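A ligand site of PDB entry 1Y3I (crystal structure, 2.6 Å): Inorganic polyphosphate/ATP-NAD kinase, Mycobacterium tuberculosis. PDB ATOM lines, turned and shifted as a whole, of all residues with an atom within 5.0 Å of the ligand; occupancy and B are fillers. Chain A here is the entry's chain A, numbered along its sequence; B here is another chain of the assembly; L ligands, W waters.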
ATOM      1  N   ASP A  85       9.538 -14.892 -29.044  1.00  0.00           N
ATOM      2  CA  ASP A  85       9.151 -15.913 -28.080  1.00  0.00           C
ATOM      3  C   ASP A  85       7.666 -16.222 -28.175  1.00  0.00           C
ATOM      4  O   ASP A  85       7.254 -17.371 -28.086  1.00  0.00           O
ATOM      5  CB  ASP A  85       9.518 -15.503 -26.650  1.00  0.00           C
ATOM      6  CG  ASP A  85      10.999 -15.674 -26.365  1.00  0.00           C
ATOM      7  OD1 ASP A  85      11.418 -15.928 -25.228  1.00  0.00           O
ATOM      8  OD2 ASP A  85      11.779 -15.538 -27.337  1.00  0.00           O
ATOM      9  N   GLY A  86       6.835 -15.206 -28.371  1.00  0.00           N
ATOM     10  CA  GLY A  86       5.398 -15.428 -28.479  1.00  0.00           C
ATOM     11  C   GLY A  86       4.987 -15.845 -29.876  1.00  0.00           C
ATOM     12  O   GLY A  86       3.817 -16.166 -30.103  1.00  0.00           O
ATOM     13  N   LEU A  89       5.720 -19.638 -29.568  1.00  0.00           N
ATOM     14  CA  LEU A  89       4.624 -20.176 -28.765  1.00  0.00           C
ATOM     15  C   LEU A  89       3.344 -20.211 -29.602  1.00  0.00           C
ATOM     16  O   LEU A  89       2.514 -21.099 -29.385  1.00  0.00           O
ATOM     17  CB  LEU A  89       4.462 -19.381 -27.476  1.00  0.00           C
ATOM     18  CG  LEU A  89       5.737 -19.227 -26.643  1.00  0.00           C
ATOM     19  CD1 LEU A  89       5.605 -18.077 -25.649  1.00  0.00           C
ATOM     20  CD2 LEU A  89       6.077 -20.519 -25.926  1.00  0.00           C
ATOM     21  N   ARG A 109      15.284  -8.160 -31.246  1.00  0.00           N
ATOM     22  CA  ARG A 109      15.035  -8.076 -29.821  1.00  0.00           C
ATOM     23  C   ARG A 109      15.055  -9.479 -29.195  1.00  0.00           C
ATOM     24  O   ARG A 109      14.249 -10.315 -29.609  1.00  0.00           O
ATOM     25  CB  ARG A 109      13.690  -7.414 -29.544  1.00  0.00           C
ATOM     26  CG  ARG A 109      13.433  -6.979 -28.105  1.00  0.00           C
ATOM     27  CD  ARG A 109      12.811  -8.059 -27.248  1.00  0.00           C
ATOM     28  NE  ARG A 109      11.518  -8.528 -27.714  1.00  0.00           N
ATOM     29  CZ  ARG A 109      10.848  -9.542 -27.167  1.00  0.00           C
ATOM     30  NH1 ARG A 109      11.368 -10.188 -26.136  1.00  0.00           N
ATOM     31  NH2 ARG A 109       9.671  -9.901 -27.650  1.00  0.00           N
ATOM     32  N   ILE A 110      15.937  -9.655 -28.235  1.00  0.00           N
ATOM     33  CA  ILE A 110      16.259 -10.856 -27.494  1.00  0.00           C
ATOM     34  C   ILE A 110      15.109 -11.870 -27.443  1.00  0.00           C
ATOM     35  O   ILE A 110      13.993 -11.527 -27.043  1.00  0.00           O
ATOM     36  CB  ILE A 110      16.682 -10.537 -26.048  1.00  0.00           C
ATOM     37  CG1 ILE A 110      17.780  -9.462 -25.940  1.00  0.00           C
ATOM     38  CG2 ILE A 110      17.117 -11.796 -25.312  1.00  0.00           C
ATOM     39  CD1 ILE A 110      18.938  -9.890 -25.057  1.00  0.00           C
ATOM     40  N   GLY A 111      15.406 -13.083 -27.879  1.00  0.00           N
ATOM     41  CA  GLY A 111      14.510 -14.225 -27.919  1.00  0.00           C
ATOM     42  C   GLY A 111      15.260 -15.504 -27.562  1.00  0.00           C
ATOM     43  O   GLY A 111      16.269 -15.809 -28.181  1.00  0.00           O
ATOM     44  N   PHE A 112      14.787 -16.240 -26.568  1.00  0.00           N
ATOM     45  CA  PHE A 112      15.538 -17.336 -25.987  1.00  0.00           C
ATOM     46  C   PHE A 112      15.591 -18.611 -26.823  1.00  0.00           C
ATOM     47  O   PHE A 112      16.683 -19.078 -27.147  1.00  0.00           O
ATOM     48  CB  PHE A 112      14.934 -17.686 -24.614  1.00  0.00           C
ATOM     49  CG  PHE A 112      15.971 -18.145 -23.592  1.00  0.00           C
ATOM     50  CD1 PHE A 112      16.782 -17.210 -22.970  1.00  0.00           C
ATOM     51  CD2 PHE A 112      16.109 -19.477 -23.274  1.00  0.00           C
ATOM     52  CE1 PHE A 112      17.722 -17.613 -22.040  1.00  0.00           C
ATOM     53  CE2 PHE A 112      17.049 -19.888 -22.349  1.00  0.00           C
ATOM     54  CZ  PHE A 112      17.852 -18.950 -21.732  1.00  0.00           C
ATOM     55  N   LEU A 113      14.430 -19.139 -27.132  1.00  0.00           N
ATOM     56  CA  LEU A 113      14.210 -20.426 -27.753  1.00  0.00           C
ATOM     57  C   LEU A 113      14.621 -20.488 -29.224  1.00  0.00           C
ATOM     58  O   LEU A 113      14.592 -21.579 -29.814  1.00  0.00           O
ATOM     59  CB  LEU A 113      12.719 -20.799 -27.658  1.00  0.00           C
ATOM     60  CG  LEU A 113      11.956 -20.361 -26.420  1.00  0.00           C
ATOM     61  CD1 LEU A 113      10.623 -21.098 -26.361  1.00  0.00           C
ATOM     62  CD2 LEU A 113      12.729 -20.602 -25.142  1.00  0.00           C
ATOM     63  N   ASN A 159       6.264 -23.282 -22.159  1.00  0.00           N
ATOM     64  CA  ASN A 159       7.003 -22.671 -21.053  1.00  0.00           C
ATOM     65  C   ASN A 159       6.485 -23.158 -19.708  1.00  0.00           C
ATOM     66  O   ASN A 159       7.157 -23.908 -19.004  1.00  0.00           O
ATOM     67  CB  ASN A 159       6.914 -21.141 -21.116  1.00  0.00           C
ATOM     68  CG  ASN A 159       8.046 -20.568 -21.941  1.00  0.00           C
ATOM     69  OD1 ASN A 159       9.008 -21.287 -22.202  1.00  0.00           O
ATOM     70  ND2 ASN A 159       7.918 -19.303 -22.343  1.00  0.00           N
ATOM     71  N   GLU A 160       5.265 -22.713 -19.380  1.00  0.00           N
ATOM     72  CA  GLU A 160       4.661 -23.025 -18.094  1.00  0.00           C
ATOM     73  C   GLU A 160       3.166 -22.711 -18.066  1.00  0.00           C
ATOM     74  O   GLU A 160       2.635 -22.111 -18.996  1.00  0.00           O
ATOM     75  CB  GLU A 160       5.321 -22.227 -16.968  1.00  0.00           C
ATOM     76  CG  GLU A 160       4.876 -20.755 -16.955  1.00  0.00           C
ATOM     77  CD  GLU A 160       5.747 -19.912 -17.873  1.00  0.00           C
ATOM     78  OE1 GLU A 160       6.837 -19.519 -17.406  1.00  0.00           O
ATOM     79  OE2 GLU A 160       5.352 -19.666 -19.037  1.00  0.00           O
ATOM     80  N   THR A 197      11.757 -25.731 -19.728  1.00  0.00           N
ATOM     81  CA  THR A 197      12.075 -24.698 -20.709  1.00  0.00           C
ATOM     82  C   THR A 197      11.428 -23.378 -20.304  1.00  0.00           C
ATOM     83  O   THR A 197      11.870 -22.291 -20.665  1.00  0.00           O
ATOM     84  CB  THR A 197      11.702 -25.121 -22.137  1.00  0.00           C
ATOM     85  OG1 THR A 197      10.478 -24.500 -22.554  1.00  0.00           O
ATOM     86  CG2 THR A 197      11.443 -26.625 -22.203  1.00  0.00           C
ATOM     87  N   GLY A 198      10.340 -23.457 -19.537  1.00  0.00           N
ATOM     88  CA  GLY A 198       9.651 -22.292 -19.019  1.00  0.00           C
ATOM     89  C   GLY A 198      10.253 -21.716 -17.747  1.00  0.00           C
ATOM     90  O   GLY A 198       9.819 -20.654 -17.305  1.00  0.00           O
ATOM     91  N   THR A 200      13.090 -20.416 -17.474  1.00  0.00           N
ATOM     92  CA  THR A 200      13.808 -19.225 -17.888  1.00  0.00           C
ATOM     93  C   THR A 200      12.858 -18.136 -18.387  1.00  0.00           C
ATOM     94  O   THR A 200      13.348 -17.106 -18.852  1.00  0.00           O
ATOM     95  CB  THR A 200      14.858 -19.526 -18.976  1.00  0.00           C
ATOM     96  OG1 THR A 200      14.220 -20.061 -20.157  1.00  0.00           O
ATOM     97  CG2 THR A 200      15.819 -20.590 -18.482  1.00  0.00           C
ATOM     98  N   ALA A 201      11.555 -18.375 -18.271  1.00  0.00           N
ATOM     99  CA  ALA A 201      10.547 -17.375 -18.632  1.00  0.00           C
ATOM    100  C   ALA A 201       9.888 -16.794 -17.388  1.00  0.00           C
ATOM    101  O   ALA A 201      10.596 -16.203 -16.546  1.00  0.00           O
ATOM    102  CB  ALA A 201       9.523 -17.980 -19.575  1.00  0.00           C
ATOM    103  N   TYR A 202       8.580 -16.935 -17.221  1.00  0.00           N
ATOM    104  CA  TYR A 202       7.939 -16.365 -16.039  1.00  0.00           C
ATOM    105  C   TYR A 202       8.564 -16.800 -14.718  1.00  0.00           C
ATOM    106  O   TYR A 202       8.814 -16.007 -13.823  1.00  0.00           O
ATOM    107  CB  TYR A 202       6.473 -16.754 -15.935  1.00  0.00           C
ATOM    108  CG  TYR A 202       5.590 -15.764 -15.208  1.00  0.00           C
ATOM    109  CD1 TYR A 202       5.875 -15.008 -14.091  1.00  0.00           C
ATOM    110  CD2 TYR A 202       4.348 -15.626 -15.786  1.00  0.00           C
ATOM    111  CE1 TYR A 202       4.951 -14.143 -13.545  1.00  0.00           C
ATOM    112  CE2 TYR A 202       3.413 -14.760 -15.261  1.00  0.00           C
ATOM    113  CZ  TYR A 202       3.715 -14.018 -14.140  1.00  0.00           C
ATOM    114  OH  TYR A 202       2.782 -13.159 -13.603  1.00  0.00           O
ATOM    115  N   ALA A 203       8.771 -18.110 -14.582  1.00  0.00           N
ATOM    116  CA  ALA A 203       9.235 -18.666 -13.324  1.00  0.00           C
ATOM    117  C   ALA A 203      10.532 -18.029 -12.869  1.00  0.00           C
ATOM    118  O   ALA A 203      10.743 -17.807 -11.685  1.00  0.00           O
ATOM    119  CB  ALA A 203       9.393 -20.182 -13.447  1.00  0.00           C
ATOM    120  N   SER A 205      11.588 -14.929 -13.463  1.00  0.00           N
ATOM    121  CA  SER A 205      11.201 -13.629 -12.935  1.00  0.00           C
ATOM    122  C   SER A 205      10.509 -13.780 -11.583  1.00  0.00           C
ATOM    123  O   SER A 205      10.721 -12.989 -10.663  1.00  0.00           O
ATOM    124  CB  SER A 205      10.249 -12.886 -13.873  1.00  0.00           C
ATOM    125  OG  SER A 205      10.789 -12.793 -15.178  1.00  0.00           O
ATOM    126  N   ASP A 257       1.313 -20.969 -21.686  1.00  0.00           N
ATOM    127  CA  ASP A 257       2.278 -20.255 -22.486  1.00  0.00           C
ATOM    128  C   ASP A 257       1.983 -18.762 -22.475  1.00  0.00           C
ATOM    129  O   ASP A 257       2.369 -18.039 -23.404  1.00  0.00           O
ATOM    130  CB  ASP A 257       2.298 -20.745 -23.937  1.00  0.00           C
ATOM    131  CG  ASP A 257       2.701 -22.200 -24.038  1.00  0.00           C
ATOM    132  OD1 ASP A 257       2.592 -22.920 -23.029  1.00  0.00           O
ATOM    133  OD2 ASP A 257       3.116 -22.578 -25.142  1.00  0.00           O
ATOM    134  N   GLY A 258       1.283 -18.288 -21.443  1.00  0.00           N
ATOM    135  CA  GLY A 258       0.884 -16.899 -21.348  1.00  0.00           C
ATOM    136  C   GLY A 258      -0.348 -16.587 -22.187  1.00  0.00           C
ATOM    137  O   GLY A 258      -1.127 -15.677 -21.905  1.00  0.00           O
ATOM    138  N   LYS B 165       1.360  -3.755 -14.148  1.00  0.00           N
ATOM    139  CA  LYS B 165       1.101  -3.845 -15.578  1.00  0.00           C
ATOM    140  C   LYS B 165      -0.384  -4.032 -15.862  1.00  0.00           C
ATOM    141  O   LYS B 165      -1.113  -4.375 -14.915  1.00  0.00           O
ATOM    142  CB  LYS B 165       1.868  -5.046 -16.154  1.00  0.00           C
ATOM    143  CG  LYS B 165       1.141  -6.369 -16.051  1.00  0.00           C
ATOM    144  CD  LYS B 165       2.039  -7.528 -15.629  1.00  0.00           C
ATOM    145  CE  LYS B 165       1.449  -8.884 -15.933  1.00  0.00           C
ATOM    146  NZ  LYS B 165       0.014  -9.020 -15.570  1.00  0.00           N
ATOM    147  N   GLY B 170       1.017  -8.492 -20.783  1.00  0.00           N
ATOM    148  CA  GLY B 170       2.252  -9.228 -20.570  1.00  0.00           C
ATOM    149  C   GLY B 170       3.212  -8.423 -19.711  1.00  0.00           C
ATOM    150  O   GLY B 170       2.830  -7.435 -19.083  1.00  0.00           O
ATOM    151  N   VAL B 171       4.471  -8.837 -19.694  1.00  0.00           N
ATOM    152  CA  VAL B 171       5.536  -8.124 -19.000  1.00  0.00           C
ATOM    153  C   VAL B 171       5.497  -6.635 -19.294  1.00  0.00           C
ATOM    154  O   VAL B 171       5.232  -6.246 -20.433  1.00  0.00           O
ATOM    155  CB  VAL B 171       6.898  -8.715 -19.442  1.00  0.00           C
ATOM    156  CG1 VAL B 171       7.686  -7.677 -20.215  1.00  0.00           C
ATOM    157  CG2 VAL B 171       7.677  -9.200 -18.241  1.00  0.00           C
ATOM    158  N   CYS B 188       8.383  -6.604 -16.551  1.00  0.00           N
ATOM    159  CA  CYS B 188       8.104  -7.316 -15.308  1.00  0.00           C
ATOM    160  C   CYS B 188       6.624  -7.427 -15.045  1.00  0.00           C
ATOM    161  O   CYS B 188       5.833  -6.949 -15.852  1.00  0.00           O
ATOM    162  CB  CYS B 188       8.789  -6.544 -14.177  1.00  0.00           C
ATOM    163  SG  CYS B 188       8.326  -4.796 -14.200  1.00  0.00           S
ATOM    164  N   ASP B 189       6.229  -8.008 -13.921  1.00  0.00           N
ATOM    165  CA  ASP B 189       4.874  -7.779 -13.433  1.00  0.00           C
ATOM    166  C   ASP B 189       4.734  -6.294 -13.097  1.00  0.00           C
ATOM    167  O   ASP B 189       3.684  -5.697 -13.280  1.00  0.00           O
ATOM    168  CB  ASP B 189       4.555  -8.633 -12.203  1.00  0.00           C
ATOM    169  CG  ASP B 189       3.962  -9.979 -12.585  1.00  0.00           C
ATOM    170  OD1 ASP B 189       3.199 -10.549 -11.762  1.00  0.00           O
ATOM    171  OD2 ASP B 189       4.281 -10.451 -13.701  1.00  0.00           O
ATOM    172  N   ASN B 224       7.998  -9.423 -10.004  1.00  0.00           N
ATOM    173  CA  ASN B 224       8.216 -10.423 -11.042  1.00  0.00           C
ATOM    174  C   ASN B 224       8.981  -9.827 -12.228  1.00  0.00           C
ATOM    175  O   ASN B 224       8.422  -9.650 -13.306  1.00  0.00           O
ATOM    176  CB  ASN B 224       6.905 -11.062 -11.494  1.00  0.00           C
ATOM    177  CG  ASN B 224       6.185 -11.763 -10.347  1.00  0.00           C
ATOM    178  OD1 ASN B 224       6.804 -12.240  -9.393  1.00  0.00           O
ATOM    179  ND2 ASN B 224       4.859 -11.829 -10.409  1.00  0.00           N
ATOM    180  N   HIS B 226      11.729  -9.841 -15.071  1.00  0.00           N
ATOM    181  CA  HIS B 226      12.589 -10.751 -15.837  1.00  0.00           C
ATOM    182  C   HIS B 226      13.970 -10.117 -15.961  1.00  0.00           C
ATOM    183  O   HIS B 226      14.312  -9.550 -16.996  1.00  0.00           O
ATOM    184  CB  HIS B 226      11.981 -11.111 -17.183  1.00  0.00           C
ATOM    185  CG  HIS B 226      12.442 -12.418 -17.742  1.00  0.00           C
ATOM    186  ND1 HIS B 226      13.225 -12.480 -18.891  1.00  0.00           N
ATOM    187  CD2 HIS B 226      12.269 -13.705 -17.367  1.00  0.00           C
ATOM    188  CE1 HIS B 226      13.499 -13.733 -19.175  1.00  0.00           C
ATOM    189  NE2 HIS B 226      12.940 -14.501 -18.261  1.00  0.00           N
HETATM  190  P1  LIG L   1       5.536 -11.358 -23.097  1.00  0.00           P
HETATM  191  O1  LIG L   1       4.624 -12.099 -22.192  1.00  0.00           O
HETATM  192  O2  LIG L   1       5.181  -9.962 -23.455  1.00  0.00           O
HETATM  193  O3  LIG L   1       6.997 -11.336 -22.407  1.00  0.00           O
HETATM  194  C1  LIG L   1       7.770 -12.537 -22.464  1.00  0.00           C
HETATM  195  C2  LIG L   1       9.229 -12.266 -22.124  1.00  0.00           C
HETATM  196  O4  LIG L   1       9.791 -13.501 -21.675  1.00  0.00           O
HETATM  197  C3  LIG L   1       9.987 -11.863 -23.396  1.00  0.00           C
HETATM  198  O5  LIG L   1      11.145 -11.094 -23.063  1.00  0.00           O
HETATM  199  C4  LIG L   1      10.409 -13.224 -23.960  1.00  0.00           C
HETATM  200  O6  LIG L   1      11.618 -13.069 -24.705  1.00  0.00           O
HETATM  201  C5  LIG L   1      10.695 -13.979 -22.670  1.00  0.00           C
HETATM  202  N1  LIG L   1      10.483 -15.427 -22.833  1.00  0.00           N
HETATM  203  C6  LIG L   1       9.403 -16.049 -23.285  1.00  0.00           C
HETATM  204  N2  LIG L   1       9.606 -17.369 -23.171  1.00  0.00           N
HETATM  205  C7  LIG L   1      10.812 -17.573 -22.656  1.00  0.00           C
HETATM  206  C8  LIG L   1      11.574 -18.678 -22.301  1.00  0.00           C
HETATM  207  N3  LIG L   1      11.079 -19.903 -22.437  1.00  0.00           N
HETATM  208  N4  LIG L   1      12.813 -18.501 -21.807  1.00  0.00           N
HETATM  209  C9  LIG L   1      13.309 -17.294 -21.641  1.00  0.00           C
HETATM  210  N5  LIG L   1      12.618 -16.210 -21.943  1.00  0.00           N
HETATM  211  C10 LIG L   1      11.384 -16.321 -22.450  1.00  0.00           C
HETATM  212  O7  LIG L   1       5.851 -12.190 -24.431  1.00  0.00           O
HETATM  213  P2  LIG L   1       5.614 -13.716 -24.818  1.00  0.00           P
HETATM  214  O8  LIG L   1       6.463 -13.981 -26.018  1.00  0.00           O
HETATM  215  O9  LIG L   1       4.160 -13.993 -24.928  1.00  0.00           O
HETATM  216  O10 LIG L   1       6.221 -14.585 -23.604  1.00  0.00           O
HETATM  217  C11 LIG L   1       5.469 -15.684 -23.069  1.00  0.00           C
HETATM  218  C12 LIG L   1       5.912 -15.898 -21.621  1.00  0.00           C
HETATM  219  O11 LIG L   1       5.570 -14.731 -20.865  1.00  0.00           O
HETATM  220  C13 LIG L   1       5.145 -16.981 -20.871  1.00  0.00           C
HETATM  221  O12 LIG L   1       5.770 -18.255 -21.117  1.00  0.00           O
HETATM  222  C14 LIG L   1       5.389 -16.565 -19.405  1.00  0.00           C
HETATM  223  O13 LIG L   1       6.456 -17.381 -18.885  1.00  0.00           O
HETATM  224  C15 LIG L   1       5.886 -15.136 -19.521  1.00  0.00           C
HETATM  225  N6  LIG L   1       5.273 -14.206 -18.564  1.00  0.00           N
HETATM  226  C16 LIG L   1       6.106 -13.581 -17.626  1.00  0.00           C
HETATM  227  C17 LIG L   1       5.600 -12.659 -16.718  1.00  0.00           C
HETATM  228  C18 LIG L   1       6.550 -12.095 -15.661  1.00  0.00           C
HETATM  229  O14 LIG L   1       6.183 -11.815 -14.510  1.00  0.00           O
HETATM  230  N7  LIG L   1       7.806 -11.938 -16.073  1.00  0.00           N
HETATM  231  C19 LIG L   1       4.144 -12.217 -16.793  1.00  0.00           C
HETATM  232  C20 LIG L   1       3.476 -12.770 -17.883  1.00  0.00           C
HETATM  233  C21 LIG L   1       3.911 -13.892 -18.562  1.00  0.00           C
HETATM  234  O   HOH W   1       2.169 -12.946 -20.770  1.00  0.00           O
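An oxygen (O14) of the ligand lies close to the backbone carbonyl oxygen (O) of Asn 224 of chain B (3.3 Å). Leu 89 touches the ligand. Ile 110 touches the ligand. Phe 112 touches the ligand. Leu 113 touches the ligand. CB of Ala 201 touches O13 of the ligand, at 3.2 Å. O of Asp 257 touches C13 of the ligand, 3.9 Å away. Val 171 of chain B touches the ligand. His 226 of chain B touches the ligand (CE1 to N5, 3.8 Å). Hydrophobic or aromatic side chains that line the ligand: Leu 89, Phe 112, Leu 113, Ala 201, Tyr 202, Val 171 of chain B and His 226 of chain B. 19 residues have an atom within 4 Å of the ligand: Asp 85, Gly 86, Leu 89, Arg 109, Ile 110, Phe 112, Leu 113, Asn 159, Glu 160, Thr 197, Thr 200, Ala 201, Tyr 202, Ser 205, Asp 257, Val 171 of chain B, Asp 189 of chain B, Asn 224 of chain B and His 226 of chain B. Along chain A the residues within 4 Å of the ligand span positions 85 to 257. The nearest printed residue that does not touch the ligand is Gly 170 of chain B (4.1 Å).
N7 of the ligand is in hydrogen-bond range of OG of Ser 205 (3.2 Å). The side-chain carboxylate (OD1) of Asp 85 sits close to an oxygen (O6) of the ligand (2.9 Å). OE2 of Glu 160 sits at hydrogen-bond distance from O13 of the ligand (2.5 Å). The backbone NH of Gly 86 sits at hydrogen-bond distance from an oxygen (O8) of the ligand (2.7 Å). N3 of the ligand is in hydrogen-bond range of OD1 of Asn 159 (2.5 Å). The side-chain carboxylate (OD2) of Asp 189 of chain B sits close to an oxygen (O14) of the ligand, at 2.5 Å. The backbone NH (N) of Tyr 202 is in hydrogen-bond range of an oxygen (O13) of the ligand. OG1 of Thr 200 sits at hydrogen-bond distance from N4 of the ligand (2.7 Å). O of Thr 197 sits at hydrogen-bond distance from N3 of the ligand (3.1 Å). An oxygen (O5) of the ligand lies within hydrogen-bond range of the guanidinium group (NH1) of Arg 109, 3.2 Å away.
A ring nitrogen (NE2) of His 226 of chain B sits at hydrogen-bond distance from the backbone carbonyl oxygen of Thr 200. The side-chain carboxylate (OD2) of Asp 189 of chain B lies within hydrogen-bond range of the side-chain hydroxyl (OH) of Tyr 202 (3.1 Å). OD2 of Asp 85 lies within hydrogen-bond range of N of Phe 112 (3.2 Å). The side-chain hydroxyl (OG) of Ser 205 lies close to the backbone NH (N) of His 226 of chain B, 3.1 Å away. The backbone NH (N) of Lys 165 of chain B is in hydrogen-bond range of the backbone carbonyl oxygen (O) of Asp 189 of chain B (3.2 Å). The side-chain carboxylate (OD1) of Asp 189 of chain B sits at hydrogen-bond distance from the side-chain amide nitrogen (ND2) of Asn 224 of chain B (2.5 Å). A ring nitrogen (NE2) of His 226 of chain B lies close to the backbone carbonyl oxygen of Ala 201. O of Asn 159 lies close to N of Gly 198, 3.3 Å away.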
